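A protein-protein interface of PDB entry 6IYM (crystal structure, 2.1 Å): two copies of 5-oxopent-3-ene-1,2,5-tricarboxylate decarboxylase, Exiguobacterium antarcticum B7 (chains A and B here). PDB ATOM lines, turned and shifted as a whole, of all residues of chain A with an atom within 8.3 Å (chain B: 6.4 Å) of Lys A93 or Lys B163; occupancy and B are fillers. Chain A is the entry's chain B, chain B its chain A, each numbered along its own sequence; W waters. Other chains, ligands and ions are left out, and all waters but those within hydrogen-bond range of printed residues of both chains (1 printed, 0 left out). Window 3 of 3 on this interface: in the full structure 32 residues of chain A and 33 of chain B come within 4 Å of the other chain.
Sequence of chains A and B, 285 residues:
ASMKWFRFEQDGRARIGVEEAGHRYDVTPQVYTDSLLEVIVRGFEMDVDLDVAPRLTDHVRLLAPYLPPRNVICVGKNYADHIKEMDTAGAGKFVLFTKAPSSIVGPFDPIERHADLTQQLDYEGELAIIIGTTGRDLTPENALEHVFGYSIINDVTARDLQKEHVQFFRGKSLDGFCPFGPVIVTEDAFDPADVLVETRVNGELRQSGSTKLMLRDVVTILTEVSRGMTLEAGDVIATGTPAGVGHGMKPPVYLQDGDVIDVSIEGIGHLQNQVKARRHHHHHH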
ATOM      1  N   VAL A  75     -21.298 -24.095 -11.356  1.00  0.00           N
ATOM      2  CA  VAL A  75     -21.509 -23.209 -12.529  1.00  0.00           C
ATOM      3  C   VAL A  75     -20.638 -23.740 -13.674  1.00  0.00           C
ATOM      4  O   VAL A  75     -19.511 -24.206 -13.391  1.00  0.00           O
ATOM      5  CB  VAL A  75     -21.219 -21.746 -12.170  1.00  0.00           C
ATOM      6  CG1 VAL A  75     -21.484 -20.805 -13.337  1.00  0.00           C
ATOM      7  CG2 VAL A  75     -21.999 -21.311 -10.951  1.00  0.00           C
ATOM      8  N   GLY A  76     -21.202 -23.760 -14.887  1.00  0.00           N
ATOM      9  CA  GLY A  76     -20.534 -24.108 -16.155  1.00  0.00           C
ATOM     10  C   GLY A  76     -19.621 -22.971 -16.578  1.00  0.00           C
ATOM     11  O   GLY A  76     -19.159 -22.279 -15.675  1.00  0.00           O
ATOM     12  N   LYS A  77     -19.369 -22.798 -17.885  1.00  0.00           N
ATOM     13  CA  LYS A  77     -18.448 -21.777 -18.473  1.00  0.00           C
ATOM     14  C   LYS A  77     -18.701 -20.423 -17.805  1.00  0.00           C
ATOM     15  O   LYS A  77     -19.742 -19.814 -18.100  1.00  0.00           O
ATOM     16  CB  LYS A  77     -18.618 -21.673 -19.997  1.00  0.00           C
ATOM     17  CG  LYS A  77     -18.223 -22.913 -20.801  1.00  0.00           C
ATOM     18  CD  LYS A  77     -17.107 -23.770 -20.182  1.00  0.00           C
ATOM     19  CE  LYS A  77     -17.021 -25.182 -20.725  1.00  0.00           C
ATOM     20  NZ  LYS A  77     -16.100 -25.281 -21.880  1.00  0.00           N
ATOM     21  N   ASN A  78     -17.810 -20.000 -16.902  1.00  0.00           N
ATOM     22  CA  ASN A  78     -17.964 -18.725 -16.152  1.00  0.00           C
ATOM     23  C   ASN A  78     -16.674 -17.877 -16.184  1.00  0.00           C
ATOM     24  O   ASN A  78     -16.629 -16.885 -15.444  1.00  0.00           O
ATOM     25  CB  ASN A  78     -18.451 -18.997 -14.732  1.00  0.00           C
ATOM     26  CG  ASN A  78     -18.959 -17.756 -14.029  1.00  0.00           C
ATOM     27  OD1 ASN A  78     -19.603 -16.907 -14.637  1.00  0.00           O
ATOM     28  ND2 ASN A  78     -18.653 -17.632 -12.746  1.00  0.00           N
ATOM     29  N   ALA A  89     -19.518 -10.371 -22.732  1.00  0.00           N
ATOM     30  CA  ALA A  89     -19.309 -11.829 -22.854  1.00  0.00           C
ATOM     31  C   ALA A  89     -20.232 -12.500 -21.827  1.00  0.00           C
ATOM     32  O   ALA A  89     -20.778 -13.582 -22.128  1.00  0.00           O
ATOM     33  CB  ALA A  89     -17.849 -12.169 -22.645  1.00  0.00           C
ATOM     34  N   GLY A  90     -20.433 -11.835 -20.676  1.00  0.00           N
ATOM     35  CA  GLY A  90     -21.248 -12.314 -19.542  1.00  0.00           C
ATOM     36  C   GLY A  90     -22.601 -12.822 -19.996  1.00  0.00           C
ATOM     37  O   GLY A  90     -23.071 -13.801 -19.398  1.00  0.00           O
ATOM     38  N   ALA A  91     -23.159 -12.207 -21.050  1.00  0.00           N
ATOM     39  CA  ALA A  91     -24.512 -12.433 -21.622  1.00  0.00           C
ATOM     40  C   ALA A  91     -24.695 -13.873 -22.133  1.00  0.00           C
ATOM     41  O   ALA A  91     -25.695 -14.108 -22.846  1.00  0.00           O
ATOM     42  CB  ALA A  91     -24.746 -11.441 -22.735  1.00  0.00           C
ATOM     43  N   GLY A  92     -23.773 -14.794 -21.817  1.00  0.00           N
ATOM     44  CA  GLY A  92     -23.925 -16.244 -22.060  1.00  0.00           C
ATOM     45  C   GLY A  92     -24.954 -16.878 -21.123  1.00  0.00           C
ATOM     46  O   GLY A  92     -25.438 -16.209 -20.177  1.00  0.00           O
ATOM     47  N   LYS A  93     -25.301 -18.134 -21.382  1.00  0.00           N
ATOM     48  CA  LYS A  93     -26.273 -18.891 -20.561  1.00  0.00           C
ATOM     49  C   LYS A  93     -25.637 -19.212 -19.204  1.00  0.00           C
ATOM     50  O   LYS A  93     -24.441 -19.474 -19.168  1.00  0.00           O
ATOM     51  CB  LYS A  93     -26.718 -20.145 -21.311  1.00  0.00           C
ATOM     52  CG  LYS A  93     -27.691 -19.863 -22.442  1.00  0.00           C
ATOM     53  CD  LYS A  93     -28.333 -21.095 -23.001  1.00  0.00           C
ATOM     54  CE  LYS A  93     -28.905 -20.860 -24.382  1.00  0.00           C
ATOM     55  NZ  LYS A  93     -30.057 -21.748 -24.644  1.00  0.00           N
ATOM     56  N   PHE A  94     -26.438 -19.116 -18.147  1.00  0.00           N
ATOM     57  CA  PHE A  94     -26.114 -19.457 -16.746  1.00  0.00           C
ATOM     58  C   PHE A  94     -26.297 -20.962 -16.556  1.00  0.00           C
ATOM     59  O   PHE A  94     -27.404 -21.394 -16.327  1.00  0.00           O
ATOM     60  CB  PHE A  94     -26.994 -18.614 -15.825  1.00  0.00           C
ATOM     61  CG  PHE A  94     -26.632 -18.708 -14.366  1.00  0.00           C
ATOM     62  CD1 PHE A  94     -25.310 -18.811 -13.969  1.00  0.00           C
ATOM     63  CD2 PHE A  94     -27.613 -18.682 -13.392  1.00  0.00           C
ATOM     64  CE1 PHE A  94     -24.976 -18.900 -12.629  1.00  0.00           C
ATOM     65  CE2 PHE A  94     -27.275 -18.759 -12.053  1.00  0.00           C
ATOM     66  CZ  PHE A  94     -25.964 -18.869 -11.678  1.00  0.00           C
ATOM     67  N   VAL A  95     -25.243 -21.751 -16.712  1.00  0.00           N
ATOM     68  CA  VAL A  95     -25.363 -23.236 -16.701  1.00  0.00           C
ATOM     69  C   VAL A  95     -25.127 -23.694 -15.268  1.00  0.00           C
ATOM     70  O   VAL A  95     -24.088 -23.283 -14.703  1.00  0.00           O
ATOM     71  CB  VAL A  95     -24.417 -23.896 -17.714  1.00  0.00           C
ATOM     72  CG1 VAL A  95     -24.441 -25.419 -17.627  1.00  0.00           C
ATOM     73  CG2 VAL A  95     -24.756 -23.436 -19.128  1.00  0.00           C
ATOM     74  N   LEU A  96     -26.079 -24.452 -14.708  1.00  0.00           N
ATOM     75  CA  LEU A  96     -26.056 -24.947 -13.297  1.00  0.00           C
ATOM     76  C   LEU A  96     -26.265 -26.466 -13.268  1.00  0.00           C
ATOM     77  O   LEU A  96     -27.238 -26.945 -13.874  1.00  0.00           O
ATOM     78  CB  LEU A  96     -27.168 -24.261 -12.500  1.00  0.00           C
ATOM     79  CG  LEU A  96     -26.863 -22.884 -11.920  1.00  0.00           C
ATOM     80  CD1 LEU A  96     -28.098 -22.337 -11.225  1.00  0.00           C
ATOM     81  CD2 LEU A  96     -25.695 -22.921 -10.944  1.00  0.00           C
ATOM     82  N   LEU A 215     -17.436 -14.339 -15.595  1.00  0.00           N
ATOM     83  CA  LEU A 215     -18.503 -13.754 -16.451  1.00  0.00           C
ATOM     84  C   LEU A 215     -19.637 -13.250 -15.566  1.00  0.00           C
ATOM     85  O   LEU A 215     -20.165 -12.190 -15.861  1.00  0.00           O
ATOM     86  CB  LEU A 215     -18.968 -14.803 -17.470  1.00  0.00           C
ATOM     87  CG  LEU A 215     -17.923 -15.205 -18.512  1.00  0.00           C
ATOM     88  CD1 LEU A 215     -18.480 -16.224 -19.507  1.00  0.00           C
ATOM     89  CD2 LEU A 215     -17.402 -13.983 -19.262  1.00  0.00           C
ATOM     90  N   ARG A 216     -19.971 -14.004 -14.518  1.00  0.00           N
ATOM     91  CA  ARG A 216     -20.873 -13.613 -13.404  1.00  0.00           C
ATOM     92  C   ARG A 216     -20.067 -13.714 -12.110  1.00  0.00           C
ATOM     93  O   ARG A 216     -19.450 -14.796 -11.908  1.00  0.00           O
ATOM     94  CB  ARG A 216     -22.091 -14.545 -13.353  1.00  0.00           C
ATOM     95  CG  ARG A 216     -22.931 -14.546 -14.627  1.00  0.00           C
ATOM     96  CD  ARG A 216     -24.063 -15.571 -14.621  1.00  0.00           C
ATOM     97  NE  ARG A 216     -25.049 -15.248 -15.648  1.00  0.00           N
ATOM     98  CZ  ARG A 216     -24.990 -15.608 -16.932  1.00  0.00           C
ATOM     99  NH1 ARG A 216     -24.009 -16.376 -17.383  1.00  0.00           N
ATOM    100  NH2 ARG A 216     -25.938 -15.208 -17.767  1.00  0.00           N
ATOM    101  N   GLU A 224     -28.771 -14.991  -8.778  1.00  0.00           N
ATOM    102  CA  GLU A 224     -29.370 -15.771  -9.886  1.00  0.00           C
ATOM    103  C   GLU A 224     -29.682 -17.205  -9.427  1.00  0.00           C
ATOM    104  O   GLU A 224     -30.729 -17.705  -9.851  1.00  0.00           O
ATOM    105  CB  GLU A 224     -28.464 -15.681 -11.108  1.00  0.00           C
ATOM    106  CG  GLU A 224     -28.517 -14.301 -11.749  1.00  0.00           C
ATOM    107  CD  GLU A 224     -27.846 -14.169 -13.108  1.00  0.00           C
ATOM    108  OE1 GLU A 224     -27.593 -15.217 -13.755  1.00  0.00           O
ATOM    109  OE2 GLU A 224     -27.548 -13.019 -13.505  1.00  0.00           O
ATOM    110  N   ALA B 158     -39.934 -26.647 -15.199  1.00  0.00           N
ATOM    111  CA  ALA B 158     -40.071 -25.412 -15.992  1.00  0.00           C
ATOM    112  C   ALA B 158     -39.388 -25.667 -17.330  1.00  0.00           C
ATOM    113  O   ALA B 158     -38.162 -25.578 -17.395  1.00  0.00           O
ATOM    114  CB  ALA B 158     -39.434 -24.248 -15.258  1.00  0.00           C
ATOM    115  N   ARG B 159     -40.154 -25.985 -18.362  1.00  0.00           N
ATOM    116  CA  ARG B 159     -39.619 -26.378 -19.695  1.00  0.00           C
ATOM    117  C   ARG B 159     -38.749 -25.253 -20.291  1.00  0.00           C
ATOM    118  O   ARG B 159     -37.777 -25.586 -21.020  1.00  0.00           O
ATOM    119  CB  ARG B 159     -40.772 -26.764 -20.622  1.00  0.00           C
ATOM    120  CG  ARG B 159     -41.604 -27.933 -20.117  1.00  0.00           C
ATOM    121  CD  ARG B 159     -40.791 -29.205 -20.063  1.00  0.00           C
ATOM    122  NE  ARG B 159     -41.571 -30.344 -19.598  1.00  0.00           N
ATOM    123  CZ  ARG B 159     -41.071 -31.551 -19.304  1.00  0.00           C
ATOM    124  NH1 ARG B 159     -39.774 -31.786 -19.423  1.00  0.00           N
ATOM    125  NH2 ARG B 159     -41.872 -32.522 -18.892  1.00  0.00           N
ATOM    126  N   ASP B 160     -39.029 -23.989 -19.971  1.00  0.00           N
ATOM    127  CA  ASP B 160     -38.291 -22.820 -20.523  1.00  0.00           C
ATOM    128  C   ASP B 160     -36.959 -22.667 -19.753  1.00  0.00           C
ATOM    129  O   ASP B 160     -35.928 -22.404 -20.399  1.00  0.00           O
ATOM    130  CB  ASP B 160     -39.187 -21.567 -20.586  1.00  0.00           C
ATOM    131  CG  ASP B 160     -40.011 -21.311 -19.338  1.00  0.00           C
ATOM    132  OD1 ASP B 160     -39.845 -22.071 -18.338  1.00  0.00           O
ATOM    133  OD2 ASP B 160     -40.772 -20.328 -19.336  1.00  0.00           O
ATOM    134  N   LEU B 161     -36.945 -22.908 -18.443  1.00  0.00           N
ATOM    135  CA  LEU B 161     -35.715 -22.833 -17.611  1.00  0.00           C
ATOM    136  C   LEU B 161     -34.764 -23.980 -17.994  1.00  0.00           C
ATOM    137  O   LEU B 161     -33.504 -23.795 -17.919  1.00  0.00           O
ATOM    138  CB  LEU B 161     -36.109 -22.874 -16.131  1.00  0.00           C
ATOM    139  CG  LEU B 161     -36.568 -21.551 -15.531  1.00  0.00           C
ATOM    140  CD1 LEU B 161     -37.601 -20.880 -16.400  1.00  0.00           C
ATOM    141  CD2 LEU B 161     -37.111 -21.757 -14.134  1.00  0.00           C
ATOM    142  N   GLN B 162     -35.321 -25.116 -18.434  1.00  0.00           N
ATOM    143  CA  GLN B 162     -34.533 -26.284 -18.906  1.00  0.00           C
ATOM    144  C   GLN B 162     -33.603 -25.857 -20.046  1.00  0.00           C
ATOM    145  O   GLN B 162     -32.445 -26.279 -20.059  1.00  0.00           O
ATOM    146  CB  GLN B 162     -35.431 -27.411 -19.411  1.00  0.00           C
ATOM    147  CG  GLN B 162     -35.667 -28.536 -18.427  1.00  0.00           C
ATOM    148  CD  GLN B 162     -36.451 -29.648 -19.095  1.00  0.00           C
ATOM    149  OE1 GLN B 162     -37.565 -29.455 -19.572  1.00  0.00           O
ATOM    150  NE2 GLN B 162     -35.852 -30.823 -19.180  1.00  0.00           N
ATOM    151  N   LYS B 163     -34.111 -25.081 -20.993  1.00  0.00           N
ATOM    152  CA  LYS B 163     -33.334 -24.646 -22.170  1.00  0.00           C
ATOM    153  C   LYS B 163     -32.486 -23.429 -21.780  1.00  0.00           C
ATOM    154  O   LYS B 163     -31.338 -23.344 -22.250  1.00  0.00           O
ATOM    155  CB  LYS B 163     -34.294 -24.418 -23.340  1.00  0.00           C
ATOM    156  CG  LYS B 163     -34.914 -25.703 -23.888  1.00  0.00           C
ATOM    157  CD  LYS B 163     -35.618 -25.554 -25.223  1.00  0.00           C
ATOM    158  CE  LYS B 163     -34.698 -25.063 -26.323  1.00  0.00           C
ATOM    159  NZ  LYS B 163     -35.343 -25.136 -27.655  1.00  0.00           N
ATOM    160  N   GLU B 164     -33.016 -22.548 -20.930  1.00  0.00           N
ATOM    161  CA  GLU B 164     -32.362 -21.277 -20.509  1.00  0.00           C
ATOM    162  C   GLU B 164     -31.088 -21.568 -19.702  1.00  0.00           C
ATOM    163  O   GLU B 164     -30.163 -20.743 -19.742  1.00  0.00           O
ATOM    164  CB  GLU B 164     -33.354 -20.470 -19.678  1.00  0.00           C
ATOM    165  CG  GLU B 164     -32.835 -19.148 -19.151  1.00  0.00           C
ATOM    166  CD  GLU B 164     -33.927 -18.239 -18.588  1.00  0.00           C
ATOM    167  OE1 GLU B 164     -35.085 -18.271 -19.111  1.00  0.00           O
ATOM    168  OE2 GLU B 164     -33.631 -17.497 -17.623  1.00  0.00           O
ATOM    169  N   HIS B 165     -31.043 -22.687 -18.976  1.00  0.00           N
ATOM    170  CA  HIS B 165     -29.934 -23.022 -18.045  1.00  0.00           C
ATOM    171  C   HIS B 165     -29.218 -24.274 -18.533  1.00  0.00           C
ATOM    172  O   HIS B 165     -28.269 -24.719 -17.830  1.00  0.00           O
ATOM    173  CB  HIS B 165     -30.453 -23.121 -16.602  1.00  0.00           C
ATOM    174  CG  HIS B 165     -30.958 -21.827 -16.074  1.00  0.00           C
ATOM    175  ND1 HIS B 165     -30.131 -20.744 -15.869  1.00  0.00           N
ATOM    176  CD2 HIS B 165     -32.195 -21.418 -15.732  1.00  0.00           C
ATOM    177  CE1 HIS B 165     -30.839 -19.731 -15.397  1.00  0.00           C
ATOM    178  NE2 HIS B 165     -32.104 -20.122 -15.292  1.00  0.00           N
ATOM    179  N   VAL B 166     -29.636 -24.759 -19.712  1.00  0.00           N
ATOM    180  CA  VAL B 166     -29.082 -25.890 -20.519  1.00  0.00           C
ATOM    181  C   VAL B 166     -29.137 -27.213 -19.745  1.00  0.00           C
ATOM    182  O   VAL B 166     -29.632 -28.229 -20.320  1.00  0.00           O
ATOM    183  CB  VAL B 166     -27.661 -25.562 -20.985  1.00  0.00           C
ATOM    184  CG1 VAL B 166     -27.063 -26.695 -21.815  1.00  0.00           C
ATOM    185  CG2 VAL B 166     -27.635 -24.242 -21.730  1.00  0.00           C
ATOM    186  N   GLN B 167     -28.566 -27.247 -18.539  1.00  0.00           N
ATOM    187  CA  GLN B 167     -28.661 -28.420 -17.641  1.00  0.00           C
ATOM    188  C   GLN B 167     -29.999 -28.346 -16.917  1.00  0.00           C
ATOM    189  O   GLN B 167     -30.440 -27.236 -16.669  1.00  0.00           O
ATOM    190  CB  GLN B 167     -27.491 -28.420 -16.667  1.00  0.00           C
ATOM    191  CG  GLN B 167     -26.168 -28.511 -17.387  1.00  0.00           C
ATOM    192  CD  GLN B 167     -25.838 -29.930 -17.733  1.00  0.00           C
ATOM    193  OE1 GLN B 167     -25.897 -30.822 -16.878  1.00  0.00           O
ATOM    194  NE2 GLN B 167     -25.468 -30.133 -18.988  1.00  0.00           N
ATOM    195  N   PHE B 168     -30.622 -29.490 -16.620  1.00  0.00           N
ATOM    196  CA  PHE B 168     -32.039 -29.540 -16.167  1.00  0.00           C
ATOM    197  C   PHE B 168     -32.185 -29.053 -14.717  1.00  0.00           C
ATOM    198  O   PHE B 168     -33.302 -28.650 -14.358  1.00  0.00           O
ATOM    199  CB  PHE B 168     -32.614 -30.939 -16.402  1.00  0.00           C
ATOM    200  CG  PHE B 168     -32.702 -31.346 -17.850  1.00  0.00           C
ATOM    201  CD1 PHE B 168     -32.587 -30.418 -18.871  1.00  0.00           C
ATOM    202  CD2 PHE B 168     -32.930 -32.664 -18.182  1.00  0.00           C
ATOM    203  CE1 PHE B 168     -32.657 -30.807 -20.199  1.00  0.00           C
ATOM    204  CE2 PHE B 168     -33.018 -33.055 -19.507  1.00  0.00           C
ATOM    205  CZ  PHE B 168     -32.885 -32.124 -20.514  1.00  0.00           C
ATOM    206  N   HIS B 247     -45.808 -30.662 -22.198  1.00  0.00           N
ATOM    207  CA  HIS B 247     -44.881 -30.167 -23.249  1.00  0.00           C
ATOM    208  C   HIS B 247     -45.014 -30.990 -24.539  1.00  0.00           C
ATOM    209  O   HIS B 247     -44.699 -30.448 -25.603  1.00  0.00           O
ATOM    210  CB  HIS B 247     -43.445 -30.226 -22.733  1.00  0.00           C
ATOM    211  CG  HIS B 247     -42.474 -29.420 -23.522  1.00  0.00           C
ATOM    212  ND1 HIS B 247     -42.623 -28.055 -23.691  1.00  0.00           N
ATOM    213  CD2 HIS B 247     -41.325 -29.770 -24.137  1.00  0.00           C
ATOM    214  CE1 HIS B 247     -41.616 -27.602 -24.403  1.00  0.00           C
ATOM    215  NE2 HIS B 247     -40.806 -28.632 -24.690  1.00  0.00           N
HETATM  216  O   HOH W   1     -29.173 -18.762 -18.678  1.00  0.00           O
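The backbone carbonyl oxygen of Phe A94 sits at hydrogen-bond distance from a ring nitrogen (ND1) of His B165 (2.8 Å). NZ of Lys A93 lies within hydrogen-bond range of O of Lys B163 (3.1 Å).
The backbone carbonyl oxygen (O) of Val A95 lies within hydrogen-bond range of the backbone NH (N) of Gly A76 (2.9 Å).
Among the printed residues, merely in contact across the chains: Leu A96 with Gln B167 (3.2 Å), Val A95 with His B165 (3.5 Å), Lys A93 with Val B166 (3.5 Å), Val A95 with Gln B167 (3.5 Å), Lys A93 with Glu B164 (3.8 Å), Leu A96 with His B165 (3.8 Å) and Val A95 with Val B166 (3.96 Å).
Of chain B, only Lys B163 (3.1 Å), Glu B164 (3.8 Å) and Val B166 (3.5 Å) come within 4 Å of Lys A93. Lys B163 touches just one residue of chain A: Lys A93. Of the printed residues of chain A, His B165 touches Phe A94 (2.8 Å), Val A95 (3.5 Å) and Leu A96 (3.8 Å). Printed residues of chain A within 4 Å of Gln B167: Val A95 and Leu A96. Of the printed residues of chain B, Val A95 touches His B165 (3.5 Å), Val B166 (3.96 Å) and Gln B167 (3.5 Å). Arg B159 touches none of the printed residues of chain A. Phe B168 touches none of the printed residues of chain A.
Hydrophobic or aromatic side chains of chain A that line the printed part of chain B: Phe A94 and Val A95. Hydrophobic or aromatic side chains of chain B that line the printed part of chain A: His B165 and Val B166. Among the printed residues, no Asp or Glu carboxylate lies within 4 Å of a Lys or Arg side-chain nitrogen of the other chain.
No position is printed for both chains.
Water W1 lies within hydrogen-bond range of the backbone carbonyl oxygen (O) of Glu B164 (2.5 Å) and the backbone NH (N) of Phe A94 (2.8 Å).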
